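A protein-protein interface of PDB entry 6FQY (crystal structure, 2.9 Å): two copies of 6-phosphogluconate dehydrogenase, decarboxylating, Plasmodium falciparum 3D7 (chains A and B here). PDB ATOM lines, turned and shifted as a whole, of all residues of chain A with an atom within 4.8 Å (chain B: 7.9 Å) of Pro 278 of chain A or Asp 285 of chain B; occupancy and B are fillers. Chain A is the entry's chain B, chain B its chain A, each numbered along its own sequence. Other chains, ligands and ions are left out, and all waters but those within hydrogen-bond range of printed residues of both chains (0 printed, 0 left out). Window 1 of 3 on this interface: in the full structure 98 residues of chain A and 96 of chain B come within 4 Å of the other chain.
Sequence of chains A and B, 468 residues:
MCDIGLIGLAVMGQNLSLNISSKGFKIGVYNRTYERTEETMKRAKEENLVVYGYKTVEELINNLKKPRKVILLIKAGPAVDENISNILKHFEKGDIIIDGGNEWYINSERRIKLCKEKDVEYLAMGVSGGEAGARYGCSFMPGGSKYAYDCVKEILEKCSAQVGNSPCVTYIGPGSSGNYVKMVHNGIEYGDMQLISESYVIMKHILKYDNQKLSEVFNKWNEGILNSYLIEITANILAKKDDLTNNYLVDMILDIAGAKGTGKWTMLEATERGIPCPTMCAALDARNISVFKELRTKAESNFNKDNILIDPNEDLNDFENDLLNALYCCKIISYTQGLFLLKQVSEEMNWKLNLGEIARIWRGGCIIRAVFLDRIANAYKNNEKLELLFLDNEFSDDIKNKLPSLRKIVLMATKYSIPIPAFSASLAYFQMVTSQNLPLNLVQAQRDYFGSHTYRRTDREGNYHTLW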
ATOM      1  N   PRO A 276      -6.619  27.398 -10.450  1.00  0.00           N
ATOM      2  CA  PRO A 276      -6.452  28.259 -11.626  1.00  0.00           C
ATOM      3  C   PRO A 276      -5.135  29.016 -11.588  1.00  0.00           C
ATOM      4  O   PRO A 276      -4.719  29.531 -10.548  1.00  0.00           O
ATOM      5  CB  PRO A 276      -7.647  29.212 -11.530  1.00  0.00           C
ATOM      6  CG  PRO A 276      -7.893  29.313 -10.063  1.00  0.00           C
ATOM      7  CD  PRO A 276      -7.589  27.954  -9.491  1.00  0.00           C
ATOM      8  N   CYS A 277      -4.482  29.082 -12.745  1.00  0.00           N
ATOM      9  CA  CYS A 277      -3.231  29.825 -12.910  1.00  0.00           C
ATOM     10  C   CYS A 277      -3.287  30.585 -14.227  1.00  0.00           C
ATOM     11  O   CYS A 277      -2.603  30.238 -15.197  1.00  0.00           O
ATOM     12  CB  CYS A 277      -2.028  28.881 -12.860  1.00  0.00           C
ATOM     13  SG  CYS A 277      -1.728  28.143 -11.233  1.00  0.00           S
ATOM     14  N   PRO A 278      -4.112  31.636 -14.300  1.00  0.00           N
ATOM     15  CA  PRO A 278      -4.299  32.320 -15.592  1.00  0.00           C
ATOM     16  C   PRO A 278      -3.036  32.991 -16.103  1.00  0.00           C
ATOM     17  O   PRO A 278      -2.785  32.982 -17.316  1.00  0.00           O
ATOM     18  CB  PRO A 278      -5.408  33.342 -15.290  1.00  0.00           C
ATOM     19  CG  PRO A 278      -6.035  32.881 -14.005  1.00  0.00           C
ATOM     20  CD  PRO A 278      -4.932  32.237 -13.236  1.00  0.00           C
ATOM     21  N   THR A 279      -2.244  33.592 -15.212  1.00  0.00           N
ATOM     22  CA  THR A 279      -0.982  34.194 -15.630  1.00  0.00           C
ATOM     23  C   THR A 279      -0.085  33.164 -16.306  1.00  0.00           C
ATOM     24  O   THR A 279       0.610  33.475 -17.281  1.00  0.00           O
ATOM     25  CB  THR A 279      -0.279  34.823 -14.425  1.00  0.00           C
ATOM     26  OG1 THR A 279      -1.043  35.943 -13.959  1.00  0.00           O
ATOM     27  CG2 THR A 279       1.118  35.295 -14.796  1.00  0.00           C
ATOM     28  N   MET A 280      -0.105  31.923 -15.814  1.00  0.00           N
ATOM     29  CA  MET A 280       0.674  30.860 -16.434  1.00  0.00           C
ATOM     30  C   MET A 280       0.010  30.342 -17.704  1.00  0.00           C
ATOM     31  O   MET A 280       0.707  29.903 -18.627  1.00  0.00           O
ATOM     32  CB  MET A 280       0.884  29.715 -15.442  1.00  0.00           C
ATOM     33  CG  MET A 280       2.345  29.383 -15.177  1.00  0.00           C
ATOM     34  SD  MET A 280       3.192  28.749 -16.638  1.00  0.00           S
ATOM     35  CE  MET A 280       2.260  27.251 -16.946  1.00  0.00           C
ATOM     36  N   CYS A 281      -1.324  30.376 -17.768  1.00  0.00           N
ATOM     37  CA  CYS A 281      -2.020  29.962 -18.983  1.00  0.00           C
ATOM     38  C   CYS A 281      -1.679  30.876 -20.151  1.00  0.00           C
ATOM     39  O   CYS A 281      -1.437  30.406 -21.267  1.00  0.00           O
ATOM     40  CB  CYS A 281      -3.530  29.942 -18.743  1.00  0.00           C
ATOM     41  SG  CYS A 281      -4.461  28.857 -19.857  1.00  0.00           S
ATOM     42  N   ALA A 282      -1.655  32.189 -19.910  1.00  0.00           N
ATOM     43  CA  ALA A 282      -1.309  33.130 -20.970  1.00  0.00           C
ATOM     44  C   ALA A 282       0.133  32.953 -21.425  1.00  0.00           C
ATOM     45  O   ALA A 282       0.443  33.131 -22.608  1.00  0.00           O
ATOM     46  CB  ALA A 282      -1.554  34.560 -20.496  1.00  0.00           C
ATOM     47  N   GLN A 337      -0.925  33.100  -7.391  1.00  0.00           N
ATOM     48  CA  GLN A 337      -1.392  31.847  -7.975  1.00  0.00           C
ATOM     49  C   GLN A 337      -0.347  30.749  -7.835  1.00  0.00           C
ATOM     50  O   GLN A 337      -0.699  29.577  -7.657  1.00  0.00           O
ATOM     51  CB  GLN A 337      -1.756  32.039  -9.447  1.00  0.00           C
ATOM     52  CG  GLN A 337      -2.517  33.314  -9.758  1.00  0.00           C
ATOM     53  CD  GLN A 337      -2.416  33.702 -11.220  1.00  0.00           C
ATOM     54  OE1 GLN A 337      -1.938  32.926 -12.047  1.00  0.00           O
ATOM     55  NE2 GLN A 337      -2.873  34.903 -11.547  1.00  0.00           N
ATOM     56  N   ALA A 425      -5.517  38.537 -18.052  1.00  0.00           N
ATOM     57  CA  ALA A 425      -5.820  37.437 -17.144  1.00  0.00           C
ATOM     58  C   ALA A 425      -5.531  37.819 -15.698  1.00  0.00           C
ATOM     59  O   ALA A 425      -6.303  37.482 -14.793  1.00  0.00           O
ATOM     60  CB  ALA A 425      -5.026  36.192 -17.539  1.00  0.00           C
ATOM     61  N   TYR A 429      -8.266  37.578 -13.026  1.00  0.00           N
ATOM     62  CA  TYR A 429      -8.096  36.674 -11.892  1.00  0.00           C
ATOM     63  C   TYR A 429      -8.315  37.397 -10.570  1.00  0.00           C
ATOM     64  O   TYR A 429      -8.952  36.858  -9.657  1.00  0.00           O
ATOM     65  CB  TYR A 429      -6.706  36.034 -11.938  1.00  0.00           C
ATOM     66  CG  TYR A 429      -6.305  35.311 -10.670  1.00  0.00           C
ATOM     67  CD1 TYR A 429      -6.646  33.979 -10.469  1.00  0.00           C
ATOM     68  CD2 TYR A 429      -5.573  35.956  -9.679  1.00  0.00           C
ATOM     69  CE1 TYR A 429      -6.276  33.313  -9.313  1.00  0.00           C
ATOM     70  CE2 TYR A 429      -5.202  35.301  -8.521  1.00  0.00           C
ATOM     71  CZ  TYR A 429      -5.555  33.981  -8.342  1.00  0.00           C
ATOM     72  OH  TYR A 429      -5.185  33.326  -7.190  1.00  0.00           O
ATOM     73  N   GLN B 194     -19.675  29.868 -20.327  1.00  0.00           N
ATOM     74  CA  GLN B 194     -18.945  30.970 -19.708  1.00  0.00           C
ATOM     75  C   GLN B 194     -19.202  32.285 -20.434  1.00  0.00           C
ATOM     76  O   GLN B 194     -19.381  33.327 -19.794  1.00  0.00           O
ATOM     77  CB  GLN B 194     -17.448  30.656 -19.675  1.00  0.00           C
ATOM     78  CG  GLN B 194     -16.597  31.730 -19.007  1.00  0.00           C
ATOM     79  CD  GLN B 194     -16.957  31.954 -17.547  1.00  0.00           C
ATOM     80  OE1 GLN B 194     -17.511  31.073 -16.888  1.00  0.00           O
ATOM     81  NE2 GLN B 194     -16.643  33.139 -17.037  1.00  0.00           N
ATOM     82  N   ALA B 257     -19.825  26.065  -9.005  1.00  0.00           N
ATOM     83  CA  ALA B 257     -20.006  25.147 -10.127  1.00  0.00           C
ATOM     84  C   ALA B 257     -18.640  24.563 -10.471  1.00  0.00           C
ATOM     85  O   ALA B 257     -17.848  25.196 -11.175  1.00  0.00           O
ATOM     86  CB  ALA B 257     -20.630  25.853 -11.327  1.00  0.00           C
ATOM     87  N   MET B 267      -8.630  20.637 -21.676  1.00  0.00           N
ATOM     88  CA  MET B 267      -7.509  21.517 -21.365  1.00  0.00           C
ATOM     89  C   MET B 267      -6.225  20.729 -21.146  1.00  0.00           C
ATOM     90  O   MET B 267      -5.133  21.238 -21.423  1.00  0.00           O
ATOM     91  CB  MET B 267      -7.829  22.369 -20.138  1.00  0.00           C
ATOM     92  CG  MET B 267      -8.005  23.849 -20.445  1.00  0.00           C
ATOM     93  SD  MET B 267      -6.548  24.589 -21.212  1.00  0.00           S
ATOM     94  CE  MET B 267      -5.613  25.087 -19.768  1.00  0.00           C
ATOM     95  N   PRO B 278      -7.566  29.375 -25.238  1.00  0.00           N
ATOM     96  CA  PRO B 278      -7.723  30.357 -24.151  1.00  0.00           C
ATOM     97  C   PRO B 278      -9.156  30.522 -23.679  1.00  0.00           C
ATOM     98  O   PRO B 278      -9.384  30.707 -22.477  1.00  0.00           O
ATOM     99  CB  PRO B 278      -7.173  31.654 -24.768  1.00  0.00           C
ATOM    100  CG  PRO B 278      -6.385  31.219 -25.974  1.00  0.00           C
ATOM    101  CD  PRO B 278      -7.080  30.000 -26.478  1.00  0.00           C
ATOM    102  N   THR B 279     -10.130  30.481 -24.593  1.00  0.00           N
ATOM    103  CA  THR B 279     -11.530  30.590 -24.193  1.00  0.00           C
ATOM    104  C   THR B 279     -11.894  29.512 -23.179  1.00  0.00           C
ATOM    105  O   THR B 279     -12.660  29.760 -22.240  1.00  0.00           O
ATOM    106  CB  THR B 279     -12.433  30.506 -25.426  1.00  0.00           C
ATOM    107  OG1 THR B 279     -12.225  31.661 -26.249  1.00  0.00           O
ATOM    108  CG2 THR B 279     -13.900  30.445 -25.023  1.00  0.00           C
ATOM    109  N   MET B 280     -11.329  28.315 -23.339  1.00  0.00           N
ATOM    110  CA  MET B 280     -11.591  27.232 -22.399  1.00  0.00           C
ATOM    111  C   MET B 280     -10.801  27.384 -21.103  1.00  0.00           C
ATOM    112  O   MET B 280     -11.270  26.946 -20.048  1.00  0.00           O
ATOM    113  CB  MET B 280     -11.300  25.892 -23.075  1.00  0.00           C
ATOM    114  CG  MET B 280     -12.285  25.584 -24.199  1.00  0.00           C
ATOM    115  SD  MET B 280     -11.585  25.913 -25.830  1.00  0.00           S
ATOM    116  CE  MET B 280     -12.977  25.581 -26.909  1.00  0.00           C
ATOM    117  N   CYS B 281      -9.621  28.008 -21.151  1.00  0.00           N
ATOM    118  CA  CYS B 281      -8.872  28.254 -19.919  1.00  0.00           C
ATOM    119  C   CYS B 281      -9.647  29.175 -18.985  1.00  0.00           C
ATOM    120  O   CYS B 281      -9.714  28.932 -17.774  1.00  0.00           O
ATOM    121  CB  CYS B 281      -7.495  28.850 -20.231  1.00  0.00           C
ATOM    122  SG  CYS B 281      -6.249  28.589 -18.930  1.00  0.00           S
ATOM    123  N   ALA B 282     -10.250  30.233 -19.532  1.00  0.00           N
ATOM    124  CA  ALA B 282     -11.060  31.128 -18.711  1.00  0.00           C
ATOM    125  C   ALA B 282     -12.286  30.411 -18.158  1.00  0.00           C
ATOM    126  O   ALA B 282     -12.712  30.671 -17.026  1.00  0.00           O
ATOM    127  CB  ALA B 282     -11.477  32.352 -19.524  1.00  0.00           C
ATOM    128  N   ALA B 283     -12.868  29.505 -18.947  1.00  0.00           N
ATOM    129  CA  ALA B 283     -14.046  28.774 -18.490  1.00  0.00           C
ATOM    130  C   ALA B 283     -13.713  27.879 -17.304  1.00  0.00           C
ATOM    131  O   ALA B 283     -14.460  27.839 -16.319  1.00  0.00           O
ATOM    132  CB  ALA B 283     -14.635  27.952 -19.637  1.00  0.00           C
ATOM    133  N   LEU B 284     -12.592  27.157 -17.376  1.00  0.00           N
ATOM    134  CA  LEU B 284     -12.188  26.315 -16.256  1.00  0.00           C
ATOM    135  C   LEU B 284     -11.704  27.146 -15.074  1.00  0.00           C
ATOM    136  O   LEU B 284     -11.868  26.732 -13.921  1.00  0.00           O
ATOM    137  CB  LEU B 284     -11.096  25.340 -16.695  1.00  0.00           C
ATOM    138  CG  LEU B 284     -11.546  23.984 -17.239  1.00  0.00           C
ATOM    139  CD1 LEU B 284     -10.347  23.077 -17.454  1.00  0.00           C
ATOM    140  CD2 LEU B 284     -12.545  23.334 -16.295  1.00  0.00           C
ATOM    141  N   ASP B 285     -11.105  28.310 -15.337  1.00  0.00           N
ATOM    142  CA  ASP B 285     -10.701  29.191 -14.245  1.00  0.00           C
ATOM    143  C   ASP B 285     -11.911  29.691 -13.468  1.00  0.00           C
ATOM    144  O   ASP B 285     -11.899  29.709 -12.232  1.00  0.00           O
ATOM    145  CB  ASP B 285      -9.884  30.365 -14.782  1.00  0.00           C
ATOM    146  CG  ASP B 285      -8.508  29.947 -15.260  1.00  0.00           C
ATOM    147  OD1 ASP B 285      -8.046  28.855 -14.864  1.00  0.00           O
ATOM    148  OD2 ASP B 285      -7.887  30.707 -16.034  1.00  0.00           O
ATOM    149  N   ALA B 286     -12.967  30.100 -14.176  1.00  0.00           N
ATOM    150  CA  ALA B 286     -14.166  30.581 -13.501  1.00  0.00           C
ATOM    151  C   ALA B 286     -14.792  29.489 -12.643  1.00  0.00           C
ATOM    152  O   ALA B 286     -15.217  29.746 -11.511  1.00  0.00           O
ATOM    153  CB  ALA B 286     -15.172  31.103 -14.526  1.00  0.00           C
ATOM    154  N   ARG B 287     -14.837  28.257 -13.155  1.00  0.00           N
ATOM    155  CA  ARG B 287     -15.424  27.162 -12.390  1.00  0.00           C
ATOM    156  C   ARG B 287     -14.565  26.821 -11.178  1.00  0.00           C
ATOM    157  O   ARG B 287     -15.090  26.562 -10.089  1.00  0.00           O
ATOM    158  CB  ARG B 287     -15.603  25.939 -13.290  1.00  0.00           C
ATOM    159  CG  ARG B 287     -16.775  26.062 -14.255  1.00  0.00           C
ATOM    160  CD  ARG B 287     -16.705  25.023 -15.369  1.00  0.00           C
ATOM    161  NE  ARG B 287     -17.879  25.063 -16.239  1.00  0.00           N
ATOM    162  CZ  ARG B 287     -18.892  24.205 -16.200  1.00  0.00           C
ATOM    163  NH1 ARG B 287     -18.900  23.210 -15.324  1.00  0.00           N
ATOM    164  NH2 ARG B 287     -19.904  24.345 -17.048  1.00  0.00           N
ATOM    165  N   ASN B 288     -13.239  26.815 -11.351  1.00  0.00           N
ATOM    166  CA  ASN B 288     -12.346  26.443 -10.259  1.00  0.00           C
ATOM    167  C   ASN B 288     -12.289  27.522  -9.183  1.00  0.00           C
ATOM    168  O   ASN B 288     -12.178  27.211  -7.991  1.00  0.00           O
ATOM    169  CB  ASN B 288     -10.948  26.154 -10.804  1.00  0.00           C
ATOM    170  CG  ASN B 288     -10.872  24.832 -11.539  1.00  0.00           C
ATOM    171  OD1 ASN B 288     -11.672  23.928 -11.298  1.00  0.00           O
ATOM    172  ND2 ASN B 288      -9.903  24.709 -12.439  1.00  0.00           N
ATOM    173  N   ILE B 289     -12.357  28.795  -9.580  1.00  0.00           N
ATOM    174  CA  ILE B 289     -12.315  29.875  -8.597  1.00  0.00           C
ATOM    175  C   ILE B 289     -13.580  29.872  -7.746  1.00  0.00           C
ATOM    176  O   ILE B 289     -13.538  30.158  -6.543  1.00  0.00           O
ATOM    177  CB  ILE B 289     -12.100  31.229  -9.300  1.00  0.00           C
ATOM    178  CG1 ILE B 289     -10.679  31.322  -9.853  1.00  0.00           C
ATOM    179  CG2 ILE B 289     -12.346  32.384  -8.349  1.00  0.00           C
ATOM    180  CD1 ILE B 289     -10.371  32.631 -10.539  1.00  0.00           C
ATOM    181  N   SER B 290     -14.721  29.530  -8.351  1.00  0.00           N
ATOM    182  CA  SER B 290     -15.985  29.530  -7.621  1.00  0.00           C
ATOM    183  C   SER B 290     -15.989  28.518  -6.486  1.00  0.00           C
ATOM    184  O   SER B 290     -16.735  28.681  -5.514  1.00  0.00           O
ATOM    185  CB  SER B 290     -17.144  29.242  -8.570  1.00  0.00           C
ATOM    186  OG  SER B 290     -17.097  27.907  -9.041  1.00  0.00           O
ATOM    187  N   VAL B 291     -15.171  27.468  -6.588  1.00  0.00           N
ATOM    188  CA  VAL B 291     -15.190  26.417  -5.577  1.00  0.00           C
ATOM    189  C   VAL B 291     -14.668  26.938  -4.244  1.00  0.00           C
ATOM    190  O   VAL B 291     -15.121  26.502  -3.177  1.00  0.00           O
ATOM    191  CB  VAL B 291     -14.379  25.209  -6.088  1.00  0.00           C
ATOM    192  CG1 VAL B 291     -13.824  24.377  -4.937  1.00  0.00           C
ATOM    193  CG2 VAL B 291     -15.226  24.356  -7.019  1.00  0.00           C
ATOM    194  N   PHE B 292     -13.750  27.901  -4.274  1.00  0.00           N
ATOM    195  CA  PHE B 292     -13.246  28.543  -3.060  1.00  0.00           C
ATOM    196  C   PHE B 292     -14.159  29.699  -2.643  1.00  0.00           C
ATOM    197  O   PHE B 292     -13.760  30.862  -2.585  1.00  0.00           O
ATOM    198  CB  PHE B 292     -11.810  29.006  -3.275  1.00  0.00           C
ATOM    199  CG  PHE B 292     -10.894  27.918  -3.762  1.00  0.00           C
ATOM    200  CD1 PHE B 292     -10.293  27.047  -2.870  1.00  0.00           C
ATOM    201  CD2 PHE B 292     -10.641  27.763  -5.116  1.00  0.00           C
ATOM    202  CE1 PHE B 292      -9.454  26.042  -3.317  1.00  0.00           C
ATOM    203  CE2 PHE B 292      -9.803  26.760  -5.569  1.00  0.00           C
ATOM    204  CZ  PHE B 292      -9.209  25.898  -4.668  1.00  0.00           C
ATOM    205  N   PRO B 421     -13.137  37.129 -18.332  1.00  0.00           N
ATOM    206  CA  PRO B 421     -11.925  36.507 -18.894  1.00  0.00           C
ATOM    207  C   PRO B 421     -12.142  35.844 -20.244  1.00  0.00           C
ATOM    208  O   PRO B 421     -11.249  35.893 -21.098  1.00  0.00           O
ATOM    209  CB  PRO B 421     -11.527  35.490 -17.815  1.00  0.00           C
ATOM    210  CG  PRO B 421     -12.789  35.223 -17.061  1.00  0.00           C
ATOM    211  CD  PRO B 421     -13.515  36.529 -17.042  1.00  0.00           C
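Pro 276 of chain A touches Asp 285 of chain B (CB to OD1, 3.4 Å). Pro 276 of chain A touches Ile 289 of chain B. CG of Pro 278 of chain A touches OD2 of Asp 285 of chain B, at 3.5 Å. Met 267 of chain B touches Cys 281 of chain A. Ile 289 of chain B touches Tyr 429 of chain A (CD1 to CD1, 3.96 Å).
The side-chain sulfur of Cys 281 of chain A forms a disulfide with the side-chain sulfur of Cys 281 of chain B (2.0 Å).
Of the 10 printed residues of chain A, 4 touch a printed residue of chain B. Of the 19 printed residues of chain B, 4 touch a printed residue of chain A. Hydrophobic or aromatic side chains of chain B that line the printed part of chain A: Met 267 and Ile 289. Among the printed residues, 6 pairs touch across the chains.
Cys 281 of chain A touches its own counterpart, Cys 281 of chain B. 5 positions are printed for both chains.
Printed residues of chain B within 4 Å of Pro 276 of chain A: Asp 285 and Ile 289. Of chain B, only Asp 285 comes within 4 Å of Pro 278 of chain A. Of the printed residues of chain B, Cys 281 of chain A touches Met 267 and Cys 281. Printed residues of chain B within 4 Å of Tyr 429 of chain A: Ile 289. Printed residues of chain A within 4 Å of Cys 281 of chain B: Cys 281. Of chain A, only Pro 276 and Pro 278 come within 4 Å of Asp 285 of chain B. The nearest residue of chain B that does not touch Pro 278 of chain A is Cys 281 of chain B (5.4 Å). The nearest residue of chain A that does not touch Asp 285 of chain B is Cys 277 of chain A (4.2 Å). The nearest printed residue of chain A that does not touch Ile 289 of chain B is Pro 278 of chain A (5.6 Å).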
